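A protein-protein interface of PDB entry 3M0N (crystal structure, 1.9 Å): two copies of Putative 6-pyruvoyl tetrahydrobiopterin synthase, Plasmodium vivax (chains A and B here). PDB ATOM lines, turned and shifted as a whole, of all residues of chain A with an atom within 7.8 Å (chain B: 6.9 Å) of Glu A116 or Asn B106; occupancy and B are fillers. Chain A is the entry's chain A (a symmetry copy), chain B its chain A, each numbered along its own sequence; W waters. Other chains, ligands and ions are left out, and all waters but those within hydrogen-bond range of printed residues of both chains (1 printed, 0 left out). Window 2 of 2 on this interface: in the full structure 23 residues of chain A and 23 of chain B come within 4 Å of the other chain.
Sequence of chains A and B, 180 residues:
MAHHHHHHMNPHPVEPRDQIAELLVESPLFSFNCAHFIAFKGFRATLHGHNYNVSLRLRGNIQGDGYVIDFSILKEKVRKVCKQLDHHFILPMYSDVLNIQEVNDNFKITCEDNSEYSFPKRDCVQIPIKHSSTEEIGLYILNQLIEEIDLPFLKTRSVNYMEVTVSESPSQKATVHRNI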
ATOM      1  N   PHE A  37      -8.491   8.802  27.400  1.00  0.00           N
ATOM      2  CA  PHE A  37      -8.894   9.607  28.516  1.00  0.00           C
ATOM      3  C   PHE A  37     -10.392   9.502  28.624  1.00  0.00           C
ATOM      4  O   PHE A  37     -11.071   9.362  27.624  1.00  0.00           O
ATOM      5  CB  PHE A  37      -8.392  11.080  28.444  1.00  0.00           C
ATOM      6  CG  PHE A  37      -8.967  11.933  27.297  1.00  0.00           C
ATOM      7  CD1 PHE A  37     -10.214  12.556  27.420  1.00  0.00           C
ATOM      8  CD2 PHE A  37      -8.204  12.199  26.156  1.00  0.00           C
ATOM      9  CE1 PHE A  37     -10.716  13.386  26.391  1.00  0.00           C
ATOM     10  CE2 PHE A  37      -8.685  13.030  25.132  1.00  0.00           C
ATOM     11  CZ  PHE A  37      -9.947  13.615  25.250  1.00  0.00           C
ATOM     12  N   ARG A  44     -13.661  15.451  32.731  1.00  0.00           N
ATOM     13  CA  ARG A  44     -12.626  15.129  31.736  1.00  0.00           C
ATOM     14  C   ARG A  44     -11.331  14.714  32.454  1.00  0.00           C
ATOM     15  O   ARG A  44     -10.799  15.486  33.254  1.00  0.00           O
ATOM     16  CB  ARG A  44     -12.379  16.354  30.848  1.00  0.00           C
ATOM     17  CG  ARG A  44     -11.572  16.100  29.583  1.00  0.00           C
ATOM     18  CD  ARG A  44     -10.067  16.307  29.773  1.00  0.00           C
ATOM     19  NE  ARG A  44      -9.702  17.680  30.131  1.00  0.00           N
ATOM     20  CZ  ARG A  44      -8.448  18.112  30.277  1.00  0.00           C
ATOM     21  NH1 ARG A  44      -7.410  17.294  30.084  1.00  0.00           N
ATOM     22  NH2 ARG A  44      -8.228  19.375  30.616  1.00  0.00           N
ATOM     23  N   ASN A  99     -15.766  16.859  20.564  1.00  0.00           N
ATOM     24  CA  ASN A  99     -15.819  17.369  19.212  1.00  0.00           C
ATOM     25  C   ASN A  99     -14.581  16.832  18.512  1.00  0.00           C
ATOM     26  O   ASN A  99     -13.433  17.242  18.821  1.00  0.00           O
ATOM     27  CB  ASN A  99     -15.864  18.895  19.263  1.00  0.00           C
ATOM     28  CG  ASN A  99     -15.998  19.521  17.912  1.00  0.00           C
ATOM     29  OD1 ASN A  99     -15.212  19.249  17.007  1.00  0.00           O
ATOM     30  ND2 ASN A  99     -17.017  20.379  17.756  1.00  0.00           N
ATOM     31  N   GLN A 101     -12.516  16.419  15.134  1.00  0.00           N
ATOM     32  CA  GLN A 101     -12.300  17.100  13.852  1.00  0.00           C
ATOM     33  C   GLN A 101     -11.201  16.380  13.086  1.00  0.00           C
ATOM     34  O   GLN A 101     -10.219  15.891  13.699  1.00  0.00           O
ATOM     35  CB  GLN A 101     -11.914  18.588  14.050  1.00  0.00           C
ATOM     36  CG  GLN A 101     -11.641  19.402  12.734  1.00  0.00           C
ATOM     37  CD  GLN A 101     -11.361  20.913  12.938  1.00  0.00           C
ATOM     38  OE1 GLN A 101     -11.403  21.423  14.048  1.00  0.00           O
ATOM     39  NE2 GLN A 101     -11.082  21.621  11.841  1.00  0.00           N
ATOM     40  N   LYS A 108      -8.227  16.086  15.639  1.00  0.00           N
ATOM     41  CA  LYS A 108      -8.200  17.112  16.657  1.00  0.00           C
ATOM     42  C   LYS A 108      -9.419  16.932  17.511  1.00  0.00           C
ATOM     43  O   LYS A 108     -10.554  16.925  16.984  1.00  0.00           O
ATOM     44  CB  LYS A 108      -8.203  18.486  16.029  1.00  0.00           C
ATOM     45  CG  LYS A 108      -8.200  19.657  17.005  1.00  0.00           C
ATOM     46  CD  LYS A 108      -8.023  20.972  16.260  1.00  0.00           C
ATOM     47  CE  LYS A 108      -8.558  22.137  17.064  1.00  0.00           C
ATOM     48  NZ  LYS A 108      -8.217  23.482  16.496  1.00  0.00           N
ATOM     49  N   ILE A 109      -9.194  16.798  18.810  1.00  0.00           N
ATOM     50  CA  ILE A 109     -10.281  16.577  19.771  1.00  0.00           C
ATOM     51  C   ILE A 109     -10.397  17.761  20.724  1.00  0.00           C
ATOM     52  O   ILE A 109      -9.386  18.196  21.366  1.00  0.00           O
ATOM     53  CB  ILE A 109     -10.052  15.311  20.581  1.00  0.00           C
ATOM     54  CG1 ILE A 109      -9.922  14.122  19.643  1.00  0.00           C
ATOM     55  CG2 ILE A 109     -11.208  15.050  21.600  1.00  0.00           C
ATOM     56  CD1 ILE A 109      -9.477  12.897  20.351  1.00  0.00           C
ATOM     57  N   THR A 110     -11.602  18.319  20.779  1.00  0.00           N
ATOM     58  CA  THR A 110     -11.913  19.422  21.684  1.00  0.00           C
ATOM     59  C   THR A 110     -12.939  19.004  22.723  1.00  0.00           C
ATOM     60  O   THR A 110     -13.994  18.435  22.393  1.00  0.00           O
ATOM     61  CB  THR A 110     -12.410  20.670  20.934  1.00  0.00           C
ATOM     62  OG1 THR A 110     -11.523  20.980  19.856  1.00  0.00           O
ATOM     63  CG2 THR A 110     -12.511  21.902  21.885  1.00  0.00           C
ATOM     64  N   CYS A 111     -12.622  19.267  23.987  1.00  0.00           N
ATOM     65  CA  CYS A 111     -13.480  18.867  25.103  1.00  0.00           C
ATOM     66  C   CYS A 111     -14.416  20.007  25.536  1.00  0.00           C
ATOM     67  O   CYS A 111     -14.282  21.152  25.068  1.00  0.00           O
ATOM     68  CB  CYS A 111     -12.608  18.404  26.272  1.00  0.00           C
ATOM     69  SG  CYS A 111     -11.515  17.028  25.809  1.00  0.00           S
ATOM     70  N   ASP A 113     -14.562  21.587  28.315  1.00  0.00           N
ATOM     71  CA  ASP A 113     -13.796  22.641  29.012  1.00  0.00           C
ATOM     72  C   ASP A 113     -12.824  23.390  28.075  1.00  0.00           C
ATOM     73  O   ASP A 113     -11.988  24.176  28.536  1.00  0.00           O
ATOM     74  CB  ASP A 113     -13.046  22.056  30.222  1.00  0.00           C
ATOM     75  CG  ASP A 113     -11.946  21.048  29.830  1.00  0.00           C
ATOM     76  OD1 ASP A 113     -11.624  20.886  28.633  1.00  0.00           O
ATOM     77  OD2 ASP A 113     -11.424  20.384  30.743  1.00  0.00           O
ATOM     78  N   ASN A 114     -12.953  23.116  26.776  1.00  0.00           N
ATOM     79  CA  ASN A 114     -12.175  23.715  25.683  1.00  0.00           C
ATOM     80  C   ASN A 114     -10.737  23.213  25.570  1.00  0.00           C
ATOM     81  O   ASN A 114     -10.000  23.723  24.753  1.00  0.00           O
ATOM     82  CB  ASN A 114     -12.210  25.256  25.708  1.00  0.00           C
ATOM     83  CG  ASN A 114     -13.611  25.805  25.529  1.00  0.00           C
ATOM     84  OD1 ASN A 114     -14.109  26.529  26.385  1.00  0.00           O
ATOM     85  ND2 ASN A 114     -14.255  25.457  24.417  1.00  0.00           N
ATOM     86  N   SER A 115     -10.383  22.194  26.355  1.00  0.00           N
ATOM     87  CA  SER A 115      -9.126  21.460  26.185  1.00  0.00           C
ATOM     88  C   SER A 115      -9.051  20.856  24.786  1.00  0.00           C
ATOM     89  O   SER A 115     -10.049  20.359  24.231  1.00  0.00           O
ATOM     90  CB  SER A 115      -8.976  20.349  27.226  1.00  0.00           C
ATOM     91  OG  SER A 115      -8.954  20.880  28.536  1.00  0.00           O
ATOM     92  N   GLU A 116      -7.846  20.873  24.232  1.00  0.00           N
ATOM     93  CA  GLU A 116      -7.641  20.499  22.858  1.00  0.00           C
ATOM     94  C   GLU A 116      -6.498  19.514  22.756  1.00  0.00           C
ATOM     95  O   GLU A 116      -5.426  19.723  23.371  1.00  0.00           O
ATOM     96  CB  GLU A 116      -7.344  21.768  22.090  1.00  0.00           C
ATOM     97  CG  GLU A 116      -7.388  21.721  20.622  1.00  0.00           C
ATOM     98  CD  GLU A 116      -7.064  23.110  20.048  1.00  0.00           C
ATOM     99  OE1 GLU A 116      -5.940  23.280  19.519  1.00  0.00           O
ATOM    100  OE2 GLU A 116      -7.917  24.014  20.181  1.00  0.00           O
ATOM    101  N   TYR A 117      -6.717  18.480  21.951  1.00  0.00           N
ATOM    102  CA  TYR A 117      -5.724  17.427  21.687  1.00  0.00           C
ATOM    103  C   TYR A 117      -5.627  17.235  20.183  1.00  0.00           C
ATOM    104  O   TYR A 117      -6.596  17.446  19.432  1.00  0.00           O
ATOM    105  CB  TYR A 117      -6.146  16.078  22.288  1.00  0.00           C
ATOM    106  CG  TYR A 117      -6.331  16.098  23.756  1.00  0.00           C
ATOM    107  CD1 TYR A 117      -5.329  15.659  24.615  1.00  0.00           C
ATOM    108  CD2 TYR A 117      -7.513  16.586  24.303  1.00  0.00           C
ATOM    109  CE1 TYR A 117      -5.504  15.687  25.975  1.00  0.00           C
ATOM    110  CE2 TYR A 117      -7.696  16.619  25.630  1.00  0.00           C
ATOM    111  CZ  TYR A 117      -6.704  16.178  26.476  1.00  0.00           C
ATOM    112  OH  TYR A 117      -6.936  16.253  27.809  1.00  0.00           O
ATOM    113  N   SER A 118      -4.470  16.808  19.723  1.00  0.00           N
ATOM    114  CA  SER A 118      -4.358  16.415  18.337  1.00  0.00           C
ATOM    115  C   SER A 118      -3.391  15.246  18.181  1.00  0.00           C
ATOM    116  O   SER A 118      -2.257  15.293  18.684  1.00  0.00           O
ATOM    117  CB  SER A 118      -3.957  17.624  17.503  1.00  0.00           C
ATOM    118  OG  SER A 118      -3.760  17.286  16.148  1.00  0.00           O
ATOM    119  N   PHE A 119      -3.849  14.213  17.489  1.00  0.00           N
ATOM    120  CA  PHE A 119      -3.061  12.979  17.241  1.00  0.00           C
ATOM    121  C   PHE A 119      -3.104  12.621  15.755  1.00  0.00           C
ATOM    122  O   PHE A 119      -4.153  12.804  15.095  1.00  0.00           O
ATOM    123  CB  PHE A 119      -3.614  11.755  17.992  1.00  0.00           C
ATOM    124  CG  PHE A 119      -4.012  11.999  19.437  1.00  0.00           C
ATOM    125  CD1 PHE A 119      -3.068  12.219  20.421  1.00  0.00           C
ATOM    126  CD2 PHE A 119      -5.334  11.962  19.814  1.00  0.00           C
ATOM    127  CE1 PHE A 119      -3.473  12.417  21.750  1.00  0.00           C
ATOM    128  CE2 PHE A 119      -5.716  12.143  21.137  1.00  0.00           C
ATOM    129  CZ  PHE A 119      -4.790  12.371  22.093  1.00  0.00           C
ATOM    130  N   GLN B 101       7.191  22.340  21.108  1.00  0.00           N
ATOM    131  CA  GLN B 101       6.779  23.743  20.970  1.00  0.00           C
ATOM    132  C   GLN B 101       5.718  24.053  22.014  1.00  0.00           C
ATOM    133  O   GLN B 101       4.864  23.186  22.326  1.00  0.00           O
ATOM    134  CB  GLN B 101       6.225  24.042  19.553  1.00  0.00           C
ATOM    135  CG  GLN B 101       5.738  25.515  19.311  1.00  0.00           C
ATOM    136  CD  GLN B 101       5.286  25.831  17.862  1.00  0.00           C
ATOM    137  OE1 GLN B 101       5.359  24.991  16.976  1.00  0.00           O
ATOM    138  NE2 GLN B 101       4.826  27.064  17.636  1.00  0.00           N
ATOM    139  N   GLU B 102       5.753  25.269  22.550  1.00  0.00           N
ATOM    140  CA  GLU B 102       4.695  25.767  23.431  1.00  0.00           C
ATOM    141  C   GLU B 102       3.714  26.553  22.585  1.00  0.00           C
ATOM    142  O   GLU B 102       4.083  27.567  22.005  1.00  0.00           O
ATOM    143  CB  GLU B 102       5.251  26.692  24.506  1.00  0.00           C
ATOM    144  CG  GLU B 102       5.974  26.008  25.641  1.00  0.00           C
ATOM    145  CD  GLU B 102       6.391  27.012  26.692  1.00  0.00           C
ATOM    146  OE1 GLU B 102       7.098  27.973  26.318  1.00  0.00           O
ATOM    147  OE2 GLU B 102       5.992  26.861  27.869  1.00  0.00           O
ATOM    148  N   VAL B 103       2.468  26.076  22.487  1.00  0.00           N
ATOM    149  CA  VAL B 103       1.440  26.720  21.705  1.00  0.00           C
ATOM    150  C   VAL B 103       0.249  26.948  22.622  1.00  0.00           C
ATOM    151  O   VAL B 103      -0.403  25.986  23.031  1.00  0.00           O
ATOM    152  CB  VAL B 103       0.998  25.814  20.514  1.00  0.00           C
ATOM    153  CG1 VAL B 103      -0.223  26.386  19.784  1.00  0.00           C
ATOM    154  CG2 VAL B 103       2.162  25.565  19.559  1.00  0.00           C
ATOM    155  N   ASN B 104      -0.026  28.217  22.939  1.00  0.00           N
ATOM    156  CA  ASN B 104      -1.051  28.594  23.907  1.00  0.00           C
ATOM    157  C   ASN B 104      -0.871  27.794  25.206  1.00  0.00           C
ATOM    158  O   ASN B 104       0.172  27.893  25.834  1.00  0.00           O
ATOM    159  CB  ASN B 104      -2.440  28.450  23.280  1.00  0.00           C
ATOM    160  CG  ASN B 104      -2.610  29.348  22.055  1.00  0.00           C
ATOM    161  OD1 ASN B 104      -2.194  30.503  22.071  1.00  0.00           O
ATOM    162  ND2 ASN B 104      -3.180  28.812  20.993  1.00  0.00           N
ATOM    163  N   ASP B 105      -1.833  26.959  25.583  1.00  0.00           N
ATOM    164  CA  ASP B 105      -1.683  26.159  26.795  1.00  0.00           C
ATOM    165  C   ASP B 105      -1.393  24.696  26.515  1.00  0.00           C
ATOM    166  O   ASP B 105      -1.628  23.852  27.377  1.00  0.00           O
ATOM    167  CB  ASP B 105      -2.932  26.284  27.679  1.00  0.00           C
ATOM    168  CG  ASP B 105      -3.220  27.713  28.074  1.00  0.00           C
ATOM    169  OD1 ASP B 105      -2.286  28.451  28.453  1.00  0.00           O
ATOM    170  OD2 ASP B 105      -4.387  28.090  27.998  1.00  0.00           O
ATOM    171  N   ASN B 106      -0.868  24.411  25.323  1.00  0.00           N
ATOM    172  CA  ASN B 106      -0.504  23.063  24.906  1.00  0.00           C
ATOM    173  C   ASN B 106       1.012  22.959  24.602  1.00  0.00           C
ATOM    174  O   ASN B 106       1.670  23.961  24.338  1.00  0.00           O
ATOM    175  CB  ASN B 106      -1.186  22.679  23.621  1.00  0.00           C
ATOM    176  CG  ASN B 106      -2.643  22.258  23.838  1.00  0.00           C
ATOM    177  OD1 ASN B 106      -3.288  22.769  24.720  1.00  0.00           O
ATOM    178  ND2 ASN B 106      -3.074  21.253  23.114  1.00  0.00           N
ATOM    179  N   PHE B 107       1.494  21.728  24.624  1.00  0.00           N
ATOM    180  CA  PHE B 107       2.775  21.344  23.984  1.00  0.00           C
ATOM    181  C   PHE B 107       2.416  20.703  22.654  1.00  0.00           C
ATOM    182  O   PHE B 107       1.552  19.801  22.586  1.00  0.00           O
ATOM    183  CB  PHE B 107       3.515  20.322  24.825  1.00  0.00           C
ATOM    184  CG  PHE B 107       4.094  20.865  26.098  1.00  0.00           C
ATOM    185  CD1 PHE B 107       5.016  21.906  26.076  1.00  0.00           C
ATOM    186  CD2 PHE B 107       3.794  20.261  27.324  1.00  0.00           C
ATOM    187  CE1 PHE B 107       5.567  22.377  27.264  1.00  0.00           C
ATOM    188  CE2 PHE B 107       4.321  20.737  28.498  1.00  0.00           C
ATOM    189  CZ  PHE B 107       5.217  21.790  28.478  1.00  0.00           C
ATOM    190  N   LYS B 108       3.039  21.208  21.601  1.00  0.00           N
ATOM    191  CA  LYS B 108       2.971  20.628  20.279  1.00  0.00           C
ATOM    192  C   LYS B 108       4.272  19.930  20.024  1.00  0.00           C
ATOM    193  O   LYS B 108       5.349  20.560  20.126  1.00  0.00           O
ATOM    194  CB  LYS B 108       2.744  21.701  19.240  1.00  0.00           C
ATOM    195  CG  LYS B 108       2.676  21.217  17.795  1.00  0.00           C
ATOM    196  CD  LYS B 108       2.269  22.353  16.869  1.00  0.00           C
ATOM    197  CE  LYS B 108       2.720  22.093  15.448  1.00  0.00           C
ATOM    198  NZ  LYS B 108       2.161  23.056  14.443  1.00  0.00           N
ATOM    199  N   SER B 118      -0.410  17.208  19.751  1.00  0.00           N
ATOM    200  CA  SER B 118      -0.591  18.336  20.637  1.00  0.00           C
ATOM    201  C   SER B 118      -1.411  17.939  21.859  1.00  0.00           C
ATOM    202  O   SER B 118      -2.494  17.346  21.729  1.00  0.00           O
ATOM    203  CB  SER B 118      -1.213  19.488  19.860  1.00  0.00           C
ATOM    204  OG  SER B 118      -1.483  20.596  20.691  1.00  0.00           O
ATOM    205  N   PHE B 119      -0.888  18.269  23.032  1.00  0.00           N
ATOM    206  CA  PHE B 119      -1.530  17.956  24.333  1.00  0.00           C
ATOM    207  C   PHE B 119      -1.571  19.209  25.209  1.00  0.00           C
ATOM    208  O   PHE B 119      -0.616  20.019  25.193  1.00  0.00           O
ATOM    209  CB  PHE B 119      -0.763  16.895  25.140  1.00  0.00           C
ATOM    210  CG  PHE B 119      -0.275  15.695  24.345  1.00  0.00           C
ATOM    211  CD1 PHE B 119      -1.151  14.744  23.861  1.00  0.00           C
ATOM    212  CD2 PHE B 119       1.068  15.502  24.126  1.00  0.00           C
ATOM    213  CE1 PHE B 119      -0.660  13.636  23.152  1.00  0.00           C
ATOM    214  CE2 PHE B 119       1.537  14.391  23.438  1.00  0.00           C
ATOM    215  CZ  PHE B 119       0.677  13.470  22.953  1.00  0.00           C
ATOM    216  N   PRO B 120      -2.607  19.348  26.049  1.00  0.00           N
ATOM    217  CA  PRO B 120      -2.560  20.357  27.083  1.00  0.00           C
ATOM    218  C   PRO B 120      -1.303  20.186  27.951  1.00  0.00           C
ATOM    219  O   PRO B 120      -0.956  19.063  28.323  1.00  0.00           O
ATOM    220  CB  PRO B 120      -3.848  20.082  27.897  1.00  0.00           C
ATOM    221  CG  PRO B 120      -4.734  19.440  26.935  1.00  0.00           C
ATOM    222  CD  PRO B 120      -3.859  18.562  26.132  1.00  0.00           C
ATOM    223  N   LYS B 121      -0.614  21.279  28.233  1.00  0.00           N
ATOM    224  CA  LYS B 121       0.602  21.193  29.046  1.00  0.00           C
ATOM    225  C   LYS B 121       0.322  20.475  30.381  1.00  0.00           C
ATOM    226  O   LYS B 121       1.143  19.678  30.832  1.00  0.00           O
ATOM    227  CB  LYS B 121       1.184  22.586  29.344  1.00  0.00           C
ATOM    228  CG  LYS B 121       1.612  23.410  28.136  1.00  0.00           C
ATOM    229  CD  LYS B 121       1.974  24.835  28.585  1.00  0.00           C
ATOM    230  CE  LYS B 121       2.521  25.705  27.451  1.00  0.00           C
ATOM    231  NZ  LYS B 121       2.754  27.143  27.866  1.00  0.00           N
ATOM    232  N   ARG B 122      -0.853  20.749  30.971  1.00  0.00           N
ATOM    233  CA  ARG B 122      -1.249  20.158  32.254  1.00  0.00           C
ATOM    234  C   ARG B 122      -1.473  18.644  32.182  1.00  0.00           C
ATOM    235  O   ARG B 122      -1.437  17.968  33.210  1.00  0.00           O
ATOM    236  CB  ARG B 122      -2.501  20.846  32.817  1.00  0.00           C
ATOM    237  CG  ARG B 122      -3.788  20.587  32.027  1.00  0.00           C
ATOM    238  CD  ARG B 122      -5.025  21.127  32.744  1.00  0.00           C
ATOM    239  NE  ARG B 122      -5.400  20.341  33.924  1.00  0.00           N
ATOM    240  CZ  ARG B 122      -5.972  19.134  33.892  1.00  0.00           C
ATOM    241  NH1 ARG B 122      -6.283  18.514  35.027  1.00  0.00           N
ATOM    242  NH2 ARG B 122      -6.229  18.531  32.736  1.00  0.00           N
ATOM    243  N   CYS B 124       0.631  16.795  30.655  1.00  0.00           N
ATOM    244  CA  CYS B 124       1.997  16.295  30.451  1.00  0.00           C
ATOM    245  C   CYS B 124       2.844  16.465  31.693  1.00  0.00           C
ATOM    246  O   CYS B 124       2.649  17.408  32.462  1.00  0.00           O
ATOM    247  CB  CYS B 124       2.684  17.037  29.318  1.00  0.00           C
ATOM    248  SG  CYS B 124       1.824  16.884  27.699  1.00  0.00           S
HETATM  249  O   HOH W   1      -5.868  22.625  25.624  1.00  0.00           O
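The side-chain amide nitrogen (ND2) of Asn B106 lies within hydrogen-bond range of the backbone carbonyl oxygen (O) of Glu A116. The backbone NH (N) of Ser B118 lies within hydrogen-bond range of the backbone carbonyl oxygen (O) of Ser A118, 2.9 Å away. NH2 of Arg B122 lies close to NH2 of Arg A44 (3.0 Å).
O of Ile A109 is in hydrogen-bond range of N of Tyr A117, at 2.7 Å. The backbone carbonyl oxygen (O) of Phe B119 sits at hydrogen-bond distance from the backbone NH (N) of Phe B107. The side-chain amide nitrogen of Asn B106 lies close to the backbone carbonyl oxygen of Phe B119, at 3.4 Å. The side-chain amino group of Lys A108 is in salt-bridge range of the side-chain carboxylate of Glu A116 (3.7 Å). O of Pro B120 is in hydrogen-bond range of SG of Cys B124 (3.6 Å). The side-chain amide nitrogen (ND2) of Asn B106 sits at hydrogen-bond distance from the side-chain hydroxyl (OG) of Ser B118, at 3.0 Å.
Pro B120 touches Glu A116 (CD to O, 3.4 Å). Ser B118 touches Tyr A117. Pro B120 touches Tyr A117. Phe A119 touches Phe B119.
Printed residues of chain B within 4 Å of Arg A44: Arg B122 (3.0 Å). Glu A116 touches two residues of chain B. Printed residues of chain A within 4 Å of Ser B118: Tyr A117 and Ser A118. Printed residues of chain A within 4 Å of Phe B119: Phe A119 (3.4 Å). Printed residues of chain A within 4 Å of Pro B120: Glu A116 and Tyr A117. Lys B121 touches none of the printed residues of chain A. The nearest residue of chain B that does not touch Glu A116 is Ser B118 (4.1 Å). The nearest printed residue of chain B that does not touch Tyr A117 is Phe B119 (4.3 Å).
Hydrophobic or aromatic side chains of chain B within 4 Å of the printed part of chain A: Phe B119 and Pro B120. Printed residues of chain A that touch a printed residue of chain B: Arg A44, Glu A116, Tyr A117, Ser A118 and Phe A119.
Ser B118 touches its own counterpart, Ser A118. Phe B119 touches its own counterpart, Phe A119.
Water W1 lies within hydrogen-bond range of OD1 of Asn B106 (2.7 Å) and N of Glu A116 (3.0 Å).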
